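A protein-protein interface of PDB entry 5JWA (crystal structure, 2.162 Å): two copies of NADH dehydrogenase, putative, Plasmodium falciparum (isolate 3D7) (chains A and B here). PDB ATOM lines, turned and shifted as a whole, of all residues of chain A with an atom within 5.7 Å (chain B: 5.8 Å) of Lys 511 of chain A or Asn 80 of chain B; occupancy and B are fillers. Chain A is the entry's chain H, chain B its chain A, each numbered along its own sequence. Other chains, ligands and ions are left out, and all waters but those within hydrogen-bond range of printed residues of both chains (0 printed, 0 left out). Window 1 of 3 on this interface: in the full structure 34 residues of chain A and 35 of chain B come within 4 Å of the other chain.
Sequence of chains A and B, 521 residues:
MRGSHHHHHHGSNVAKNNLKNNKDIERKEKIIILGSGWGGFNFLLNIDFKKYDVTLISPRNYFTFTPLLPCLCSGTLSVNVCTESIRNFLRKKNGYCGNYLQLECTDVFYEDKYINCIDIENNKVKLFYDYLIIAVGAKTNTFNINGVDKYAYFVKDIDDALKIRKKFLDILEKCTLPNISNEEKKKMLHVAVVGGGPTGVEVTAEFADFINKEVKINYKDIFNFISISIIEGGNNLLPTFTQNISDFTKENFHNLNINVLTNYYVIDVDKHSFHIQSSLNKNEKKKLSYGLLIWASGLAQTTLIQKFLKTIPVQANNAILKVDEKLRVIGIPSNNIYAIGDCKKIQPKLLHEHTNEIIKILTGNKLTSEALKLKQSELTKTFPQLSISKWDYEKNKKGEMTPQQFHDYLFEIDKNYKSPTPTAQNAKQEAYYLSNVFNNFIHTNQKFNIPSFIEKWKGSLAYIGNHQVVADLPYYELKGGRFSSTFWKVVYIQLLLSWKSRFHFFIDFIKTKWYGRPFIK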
ATOM      1  N   GLY A  75     -13.578 -15.524  -9.725  1.00  0.00           N
ATOM      2  CA  GLY A  75     -12.384 -14.950 -10.308  1.00  0.00           C
ATOM      3  C   GLY A  75     -12.298 -15.100 -11.818  1.00  0.00           C
ATOM      4  O   GLY A  75     -11.248 -14.857 -12.400  1.00  0.00           O
ATOM      5  N   THR A  76     -13.389 -15.507 -12.464  1.00  0.00           N
ATOM      6  CA  THR A  76     -13.407 -15.572 -13.932  1.00  0.00           C
ATOM      7  C   THR A  76     -13.181 -14.183 -14.543  1.00  0.00           C
ATOM      8  O   THR A  76     -12.436 -14.022 -15.506  1.00  0.00           O
ATOM      9  CB  THR A  76     -14.732 -16.143 -14.460  1.00  0.00           C
ATOM     10  OG1 THR A  76     -14.845 -17.520 -14.089  1.00  0.00           O
ATOM     11  CG2 THR A  76     -14.799 -16.037 -15.970  1.00  0.00           C
ATOM     12  N   LEU A  77     -13.827 -13.180 -13.962  1.00  0.00           N
ATOM     13  CA  LEU A  77     -13.709 -11.801 -14.416  1.00  0.00           C
ATOM     14  C   LEU A  77     -13.212 -10.916 -13.269  1.00  0.00           C
ATOM     15  O   LEU A  77     -13.318 -11.288 -12.100  1.00  0.00           O
ATOM     16  CB  LEU A  77     -15.058 -11.296 -14.936  1.00  0.00           C
ATOM     17  CG  LEU A  77     -15.636 -12.013 -16.159  1.00  0.00           C
ATOM     18  CD1 LEU A  77     -17.044 -11.522 -16.446  1.00  0.00           C
ATOM     19  CD2 LEU A  77     -14.773 -11.779 -17.375  1.00  0.00           C
ATOM     20  N   SER A  78     -12.687  -9.743 -13.603  1.00  0.00           N
ATOM     21  CA  SER A  78     -12.129  -8.838 -12.597  1.00  0.00           C
ATOM     22  C   SER A  78     -13.070  -7.688 -12.257  1.00  0.00           C
ATOM     23  O   SER A  78     -14.117  -7.507 -12.877  1.00  0.00           O
ATOM     24  CB  SER A  78     -10.799  -8.270 -13.081  1.00  0.00           C
ATOM     25  OG  SER A  78     -11.003  -7.540 -14.278  1.00  0.00           O
ATOM     26  N   PHE A 506     -12.872  -8.635 -22.714  1.00  0.00           N
ATOM     27  CA  PHE A 506     -12.129  -9.411 -23.693  1.00  0.00           C
ATOM     28  C   PHE A 506     -10.852  -9.980 -23.080  1.00  0.00           C
ATOM     29  O   PHE A 506     -10.582 -11.181 -23.176  1.00  0.00           O
ATOM     30  CB  PHE A 506     -11.810  -8.533 -24.907  1.00  0.00           C
ATOM     31  CG  PHE A 506     -11.061  -9.241 -25.993  1.00  0.00           C
ATOM     32  CD1 PHE A 506     -11.733  -9.977 -26.942  1.00  0.00           C
ATOM     33  CD2 PHE A 506      -9.690  -9.149 -26.085  1.00  0.00           C
ATOM     34  CE1 PHE A 506     -11.066 -10.618 -27.950  1.00  0.00           C
ATOM     35  CE2 PHE A 506      -9.013  -9.789 -27.099  1.00  0.00           C
ATOM     36  CZ  PHE A 506      -9.707 -10.531 -28.028  1.00  0.00           C
ATOM     37  N   ILE A 507     -10.072  -9.122 -22.428  1.00  0.00           N
ATOM     38  CA  ILE A 507      -8.779  -9.535 -21.881  1.00  0.00           C
ATOM     39  C   ILE A 507      -8.932 -10.567 -20.758  1.00  0.00           C
ATOM     40  O   ILE A 507      -8.146 -11.517 -20.667  1.00  0.00           O
ATOM     41  CB  ILE A 507      -7.982  -8.312 -21.366  1.00  0.00           C
ATOM     42  CG1 ILE A 507      -7.561  -7.423 -22.534  1.00  0.00           C
ATOM     43  CG2 ILE A 507      -6.732  -8.747 -20.573  1.00  0.00           C
ATOM     44  CD1 ILE A 507      -6.729  -8.146 -23.575  1.00  0.00           C
ATOM     45  N   ASP A 508      -9.937 -10.381 -19.903  1.00  0.00           N
ATOM     46  CA  ASP A 508     -10.165 -11.309 -18.801  1.00  0.00           C
ATOM     47  C   ASP A 508     -10.457 -12.729 -19.262  1.00  0.00           C
ATOM     48  O   ASP A 508     -10.051 -13.684 -18.608  1.00  0.00           O
ATOM     49  CB  ASP A 508     -11.322 -10.839 -17.923  1.00  0.00           C
ATOM     50  CG  ASP A 508     -10.884  -9.829 -16.886  1.00  0.00           C
ATOM     51  OD1 ASP A 508      -9.700  -9.414 -16.913  1.00  0.00           O
ATOM     52  OD2 ASP A 508     -11.731  -9.444 -16.050  1.00  0.00           O
ATOM     53  N   PHE A 509     -11.160 -12.889 -20.375  1.00  0.00           N
ATOM     54  CA  PHE A 509     -11.395 -14.240 -20.846  1.00  0.00           C
ATOM     55  C   PHE A 509     -10.123 -14.854 -21.439  1.00  0.00           C
ATOM     56  O   PHE A 509      -9.868 -16.036 -21.241  1.00  0.00           O
ATOM     57  CB  PHE A 509     -12.557 -14.270 -21.841  1.00  0.00           C
ATOM     58  CG  PHE A 509     -13.901 -14.239 -21.172  1.00  0.00           C
ATOM     59  CD1 PHE A 509     -14.322 -15.318 -20.391  1.00  0.00           C
ATOM     60  CD2 PHE A 509     -14.732 -13.129 -21.292  1.00  0.00           C
ATOM     61  CE1 PHE A 509     -15.544 -15.293 -19.751  1.00  0.00           C
ATOM     62  CE2 PHE A 509     -15.959 -13.097 -20.662  1.00  0.00           C
ATOM     63  CZ  PHE A 509     -16.365 -14.181 -19.882  1.00  0.00           C
ATOM     64  N   ILE A 510      -9.311 -14.055 -22.126  1.00  0.00           N
ATOM     65  CA  ILE A 510      -7.983 -14.525 -22.536  1.00  0.00           C
ATOM     66  C   ILE A 510      -7.138 -14.938 -21.326  1.00  0.00           C
ATOM     67  O   ILE A 510      -6.572 -16.035 -21.304  1.00  0.00           O
ATOM     68  CB  ILE A 510      -7.216 -13.459 -23.322  1.00  0.00           C
ATOM     69  CG1 ILE A 510      -7.989 -13.078 -24.578  1.00  0.00           C
ATOM     70  CG2 ILE A 510      -5.798 -13.943 -23.666  1.00  0.00           C
ATOM     71  CD1 ILE A 510      -7.246 -12.071 -25.413  1.00  0.00           C
ATOM     72  N   LYS A 511      -7.067 -14.064 -20.317  1.00  0.00           N
ATOM     73  CA  LYS A 511      -6.322 -14.379 -19.102  1.00  0.00           C
ATOM     74  C   LYS A 511      -6.822 -15.691 -18.497  1.00  0.00           C
ATOM     75  O   LYS A 511      -6.030 -16.572 -18.176  1.00  0.00           O
ATOM     76  CB  LYS A 511      -6.428 -13.231 -18.084  1.00  0.00           C
ATOM     77  CG  LYS A 511      -6.641 -13.676 -16.617  1.00  0.00           C
ATOM     78  CD  LYS A 511      -7.022 -12.479 -15.696  1.00  0.00           C
ATOM     79  CE  LYS A 511      -8.254 -12.764 -14.814  1.00  0.00           C
ATOM     80  NZ  LYS A 511      -8.108 -12.143 -13.454  1.00  0.00           N
ATOM     81  N   THR A 512      -8.140 -15.825 -18.371  1.00  0.00           N
ATOM     82  CA  THR A 512      -8.712 -17.007 -17.741  1.00  0.00           C
ATOM     83  C   THR A 512      -8.461 -18.259 -18.586  1.00  0.00           C
ATOM     84  O   THR A 512      -8.165 -19.316 -18.050  1.00  0.00           O
ATOM     85  CB  THR A 512     -10.209 -16.833 -17.485  1.00  0.00           C
ATOM     86  OG1 THR A 512     -10.392 -15.719 -16.612  1.00  0.00           O
ATOM     87  CG2 THR A 512     -10.791 -18.075 -16.789  1.00  0.00           C
ATOM     88  N   LYS A 513      -8.535 -18.138 -19.904  1.00  0.00           N
ATOM     89  CA  LYS A 513      -8.248 -19.294 -20.750  1.00  0.00           C
ATOM     90  C   LYS A 513      -6.765 -19.700 -20.717  1.00  0.00           C
ATOM     91  O   LYS A 513      -6.440 -20.874 -20.613  1.00  0.00           O
ATOM     92  CB  LYS A 513      -8.672 -19.018 -22.184  1.00  0.00           C
ATOM     93  CG  LYS A 513      -8.594 -20.234 -23.095  1.00  0.00           C
ATOM     94  CD  LYS A 513      -9.044 -19.888 -24.508  1.00  0.00           C
ATOM     95  CE  LYS A 513      -8.977 -21.095 -25.442  1.00  0.00           C
ATOM     96  NZ  LYS A 513      -9.459 -20.747 -26.816  1.00  0.00           N
ATOM     97  N   TRP A 514      -5.864 -18.732 -20.805  1.00  0.00           N
ATOM     98  CA  TRP A 514      -4.442 -19.049 -20.904  1.00  0.00           C
ATOM     99  C   TRP A 514      -3.799 -19.385 -19.555  1.00  0.00           C
ATOM    100  O   TRP A 514      -2.949 -20.264 -19.484  1.00  0.00           O
ATOM    101  CB  TRP A 514      -3.672 -17.891 -21.542  1.00  0.00           C
ATOM    102  CG  TRP A 514      -3.897 -17.696 -23.009  1.00  0.00           C
ATOM    103  CD1 TRP A 514      -4.750 -18.399 -23.823  1.00  0.00           C
ATOM    104  CD2 TRP A 514      -3.267 -16.707 -23.842  1.00  0.00           C
ATOM    105  NE1 TRP A 514      -4.677 -17.910 -25.110  1.00  0.00           N
ATOM    106  CE2 TRP A 514      -3.775 -16.873 -25.147  1.00  0.00           C
ATOM    107  CE3 TRP A 514      -2.321 -15.696 -23.606  1.00  0.00           C
ATOM    108  CZ2 TRP A 514      -3.366 -16.067 -26.216  1.00  0.00           C
ATOM    109  CZ3 TRP A 514      -1.912 -14.897 -24.671  1.00  0.00           C
ATOM    110  CH2 TRP A 514      -2.434 -15.090 -25.957  1.00  0.00           C
ATOM    111  N   TYR A 515      -4.188 -18.682 -18.493  1.00  0.00           N
ATOM    112  CA  TYR A 515      -3.500 -18.830 -17.207  1.00  0.00           C
ATOM    113  C   TYR A 515      -4.383 -19.341 -16.068  1.00  0.00           C
ATOM    114  O   TYR A 515      -3.871 -19.707 -15.023  1.00  0.00           O
ATOM    115  CB  TYR A 515      -2.864 -17.497 -16.796  1.00  0.00           C
ATOM    116  CG  TYR A 515      -2.040 -16.880 -17.895  1.00  0.00           C
ATOM    117  CD1 TYR A 515      -0.863 -17.484 -18.336  1.00  0.00           C
ATOM    118  CD2 TYR A 515      -2.437 -15.697 -18.503  1.00  0.00           C
ATOM    119  CE1 TYR A 515      -0.109 -16.924 -19.366  1.00  0.00           C
ATOM    120  CE2 TYR A 515      -1.685 -15.128 -19.526  1.00  0.00           C
ATOM    121  CZ  TYR A 515      -0.525 -15.747 -19.947  1.00  0.00           C
ATOM    122  OH  TYR A 515       0.210 -15.183 -20.965  1.00  0.00           O
ATOM    123  N   GLY A 516      -5.698 -19.379 -16.259  1.00  0.00           N
ATOM    124  CA  GLY A 516      -6.575 -19.888 -15.219  1.00  0.00           C
ATOM    125  C   GLY A 516      -7.045 -18.824 -14.233  1.00  0.00           C
ATOM    126  O   GLY A 516      -6.590 -17.692 -14.262  1.00  0.00           O
ATOM    127  N   PRO A 518      -7.283 -16.925 -10.693  1.00  0.00           N
ATOM    128  CA  PRO A 518      -6.258 -16.673  -9.668  1.00  0.00           C
ATOM    129  C   PRO A 518      -6.641 -17.151  -8.257  1.00  0.00           C
ATOM    130  O   PRO A 518      -7.823 -17.298  -7.946  1.00  0.00           O
ATOM    131  CB  PRO A 518      -6.114 -15.147  -9.695  1.00  0.00           C
ATOM    132  CG  PRO A 518      -7.462 -14.657 -10.125  1.00  0.00           C
ATOM    133  CD  PRO A 518      -8.001 -15.697 -11.085  1.00  0.00           C
ATOM    134  N   ILE A 520      -5.040 -15.574  -5.461  1.00  0.00           N
ATOM    135  CA  ILE A 520      -4.679 -14.484  -4.556  1.00  0.00           C
ATOM    136  C   ILE A 520      -5.856 -14.103  -3.645  1.00  0.00           C
ATOM    137  O   ILE A 520      -6.936 -13.796  -4.144  1.00  0.00           O
ATOM    138  CB  ILE A 520      -4.224 -13.231  -5.342  1.00  0.00           C
ATOM    139  CG1 ILE A 520      -3.245 -13.626  -6.437  1.00  0.00           C
ATOM    140  CG2 ILE A 520      -3.578 -12.209  -4.409  1.00  0.00           C
ATOM    141  CD1 ILE A 520      -1.992 -14.269  -5.892  1.00  0.00           C
ATOM    142  N   SER B  78      -1.877  -3.593 -11.667  1.00  0.00           N
ATOM    143  CA  SER B  78      -2.856  -4.326 -10.876  1.00  0.00           C
ATOM    144  C   SER B  78      -2.200  -5.381  -9.997  1.00  0.00           C
ATOM    145  O   SER B  78      -0.998  -5.634 -10.095  1.00  0.00           O
ATOM    146  CB  SER B  78      -3.868  -5.002 -11.796  1.00  0.00           C
ATOM    147  OG  SER B  78      -3.196  -5.986 -12.565  1.00  0.00           O
ATOM    148  N   VAL B  79      -3.002  -6.004  -9.148  1.00  0.00           N
ATOM    149  CA  VAL B  79      -2.488  -6.975  -8.206  1.00  0.00           C
ATOM    150  C   VAL B  79      -1.933  -8.209  -8.930  1.00  0.00           C
ATOM    151  O   VAL B  79      -0.962  -8.813  -8.470  1.00  0.00           O
ATOM    152  CB  VAL B  79      -3.573  -7.386  -7.192  1.00  0.00           C
ATOM    153  CG1 VAL B  79      -3.051  -8.456  -6.218  1.00  0.00           C
ATOM    154  CG2 VAL B  79      -4.035  -6.170  -6.406  1.00  0.00           C
ATOM    155  N   ASN B  80      -2.529  -8.570 -10.065  1.00  0.00           N
ATOM    156  CA  ASN B  80      -2.074  -9.734 -10.821  1.00  0.00           C
ATOM    157  C   ASN B  80      -0.665  -9.595 -11.405  1.00  0.00           C
ATOM    158  O   ASN B  80      -0.005 -10.607 -11.650  1.00  0.00           O
ATOM    159  CB  ASN B  80      -3.044 -10.053 -11.966  1.00  0.00           C
ATOM    160  CG  ASN B  80      -4.408 -10.498 -11.471  1.00  0.00           C
ATOM    161  OD1 ASN B  80      -4.523 -11.505 -10.772  1.00  0.00           O
ATOM    162  ND2 ASN B  80      -5.454  -9.754 -11.840  1.00  0.00           N
ATOM    163  N   VAL B  81      -0.212  -8.365 -11.664  1.00  0.00           N
ATOM    164  CA  VAL B  81       1.168  -8.151 -12.106  1.00  0.00           C
ATOM    165  C   VAL B  81       2.121  -8.334 -10.935  1.00  0.00           C
ATOM    166  O   VAL B  81       3.238  -8.798 -11.106  1.00  0.00           O
ATOM    167  CB  VAL B  81       1.411  -6.740 -12.698  1.00  0.00           C
ATOM    168  CG1 VAL B  81       2.813  -6.658 -13.294  1.00  0.00           C
ATOM    169  CG2 VAL B  81       0.400  -6.425 -13.762  1.00  0.00           C
ATOM    170  N   CYS B  82       1.653  -7.980  -9.742  1.00  0.00           N
ATOM    171  CA  CYS B  82       2.500  -7.923  -8.549  1.00  0.00           C
ATOM    172  C   CYS B  82       2.529  -9.197  -7.699  1.00  0.00           C
ATOM    173  O   CYS B  82       3.125  -9.207  -6.629  1.00  0.00           O
ATOM    174  CB  CYS B  82       2.049  -6.765  -7.650  1.00  0.00           C
ATOM    175  SG  CYS B  82       2.168  -5.161  -8.435  1.00  0.00           S
ATOM    176  N   THR B  83       1.887 -10.263  -8.143  1.00  0.00           N
ATOM    177  CA  THR B  83       1.840 -11.464  -7.304  1.00  0.00           C
ATOM    178  C   THR B  83       2.027 -12.755  -8.090  1.00  0.00           C
ATOM    179  O   THR B  83       1.851 -12.779  -9.309  1.00  0.00           O
ATOM    180  CB  THR B  83       0.483 -11.585  -6.548  1.00  0.00           C
ATOM    181  OG1 THR B  83      -0.587 -11.514  -7.495  1.00  0.00           O
ATOM    182  CG2 THR B  83       0.315 -10.509  -5.501  1.00  0.00           C
ATOM    183  N   LYS B 500       2.265 -15.288 -17.165  1.00  0.00           N
ATOM    184  CA  LYS B 500       1.025 -14.697 -16.672  1.00  0.00           C
ATOM    185  C   LYS B 500       1.267 -13.231 -16.270  1.00  0.00           C
ATOM    186  O   LYS B 500       0.562 -12.324 -16.717  1.00  0.00           O
ATOM    187  CB  LYS B 500       0.482 -15.520 -15.488  1.00  0.00           C
ATOM    188  CG  LYS B 500      -0.837 -15.037 -14.878  1.00  0.00           C
ATOM    189  CD  LYS B 500      -0.633 -13.946 -13.800  1.00  0.00           C
ATOM    190  CE  LYS B 500       0.164 -14.486 -12.605  1.00  0.00           C
ATOM    191  NZ  LYS B 500       0.501 -13.427 -11.594  1.00  0.00           N
ATOM    192  N   SER B 501       2.277 -13.005 -15.441  1.00  0.00           N
ATOM    193  CA  SER B 501       2.531 -11.665 -14.931  1.00  0.00           C
ATOM    194  C   SER B 501       3.005 -10.736 -16.044  1.00  0.00           C
ATOM    195  O   SER B 501       2.700  -9.555 -16.037  1.00  0.00           O
ATOM    196  CB  SER B 501       3.554 -11.710 -13.800  1.00  0.00           C
ATOM    197  OG  SER B 501       3.051 -12.445 -12.702  1.00  0.00           O
ATOM    198  N   PHE B 503       2.133 -10.916 -19.217  1.00  0.00           N
ATOM    199  CA  PHE B 503       0.927 -10.600 -19.967  1.00  0.00           C
ATOM    200  C   PHE B 503       0.196  -9.440 -19.295  1.00  0.00           C
ATOM    201  O   PHE B 503      -0.154  -8.459 -19.941  1.00  0.00           O
ATOM    202  CB  PHE B 503       0.033 -11.845 -20.071  1.00  0.00           C
ATOM    203  CG  PHE B 503      -1.318 -11.594 -20.703  1.00  0.00           C
ATOM    204  CD1 PHE B 503      -1.483 -11.672 -22.071  1.00  0.00           C
ATOM    205  CD2 PHE B 503      -2.419 -11.302 -19.919  1.00  0.00           C
ATOM    206  CE1 PHE B 503      -2.728 -11.456 -22.648  1.00  0.00           C
ATOM    207  CE2 PHE B 503      -3.671 -11.081 -20.494  1.00  0.00           C
ATOM    208  CZ  PHE B 503      -3.818 -11.162 -21.864  1.00  0.00           C
ATOM    209  N   HIS B 504       0.003  -9.550 -17.985  1.00  0.00           N
ATOM    210  CA  HIS B 504      -0.652  -8.495 -17.210  1.00  0.00           C
ATOM    211  C   HIS B 504       0.120  -7.169 -17.182  1.00  0.00           C
ATOM    212  O   HIS B 504      -0.479  -6.097 -17.187  1.00  0.00           O
ATOM    213  CB  HIS B 504      -0.881  -8.973 -15.776  1.00  0.00           C
ATOM    214  CG  HIS B 504      -2.088  -9.836 -15.613  1.00  0.00           C
ATOM    215  ND1 HIS B 504      -3.362  -9.319 -15.517  1.00  0.00           N
ATOM    216  CD2 HIS B 504      -2.219 -11.181 -15.517  1.00  0.00           C
ATOM    217  CE1 HIS B 504      -4.227 -10.308 -15.366  1.00  0.00           C
ATOM    218  NE2 HIS B 504      -3.559 -11.448 -15.357  1.00  0.00           N
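Gly 75 of chain A touches none of the printed residues of chain B.
Lys 511 of chain A touches just these residues of chain B: Asn 80 (3.9 Å) and His 504 (3.6 Å).
Of the printed residues of chain B, Tyr 515 of chain A touches Lys 500 (3.6 Å) and Phe 503 (3.5 Å).
Of the printed residues of chain B, Ile 520 of chain A touches Thr 83 (3.5 Å).
Asn 80 of chain B touches just one residue of chain A: Lys 511 (3.9 Å).
Ser 501 of chain B touches none of the printed residues of chain A.
Printed residues of chain A within 4 Å of Phe 503 of chain B: Ile 507, Ile 510 and Tyr 515.
Printed residues of chain A within 4 Å of His 504 of chain B: Lys 511 (3.6 Å).
The nearest residue of chain B that does not touch Lys 511 of chain A is Phe 503 of chain B (4.2 Å).
Hydrophobic or aromatic side chains of chain A within 4 Å of the printed part of chain B: Ile 507, Ile 510, Tyr 515 and Ile 520.
Of the 10 printed residues of chain B, 5 touch a printed residue of chain A.
Among the printed residues, no Asp or Glu carboxylate lies within 4 Å of a Lys or Arg side-chain nitrogen of the other chain.
Among the printed residues, merely in contact across the chains: Ile 507 of chain A with Phe 503 of chain B (3.9 Å), Ile 510 of chain A with Phe 503 of chain B (3.9 Å), Lys 511 of chain A with Asn 80 of chain B (3.9 Å), Lys 511 of chain A with His 504 of chain B (3.6 Å), Tyr 515 of chain A with Lys 500 of chain B (3.6 Å), Tyr 515 of chain A with Phe 503 of chain B (3.5 Å) and Ile 520 of chain A with Thr 83 of chain B (3.5 Å).
The backbone carbonyl oxygen of Val 79 of chain B sits at hydrogen-bond distance from the side-chain hydroxyl of Thr 83 of chain B, at 2.9 Å.
N of Gly 516 of chain A sits at hydrogen-bond distance from O of Lys 511 of chain A, 3.4 Å away.
The backbone carbonyl oxygen (O) of Thr 83 of chain B lies within hydrogen-bond range of the side-chain amino group (NZ) of Lys 500 of chain B (2.7 Å).
The side-chain amino group of Lys 500 of chain B lies within hydrogen-bond range of the side-chain hydroxyl of Ser 501 of chain B (2.9 Å).
The side-chain amino group of Lys 500 of chain B is in hydrogen-bond range of the backbone carbonyl oxygen of Asn 80 of chain B, at 2.9 Å.
Position printed for both chains: 78.
Of the 7 pairs that touch across the chains among the printed residues, none has its exchanged pair printed and touching as well.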
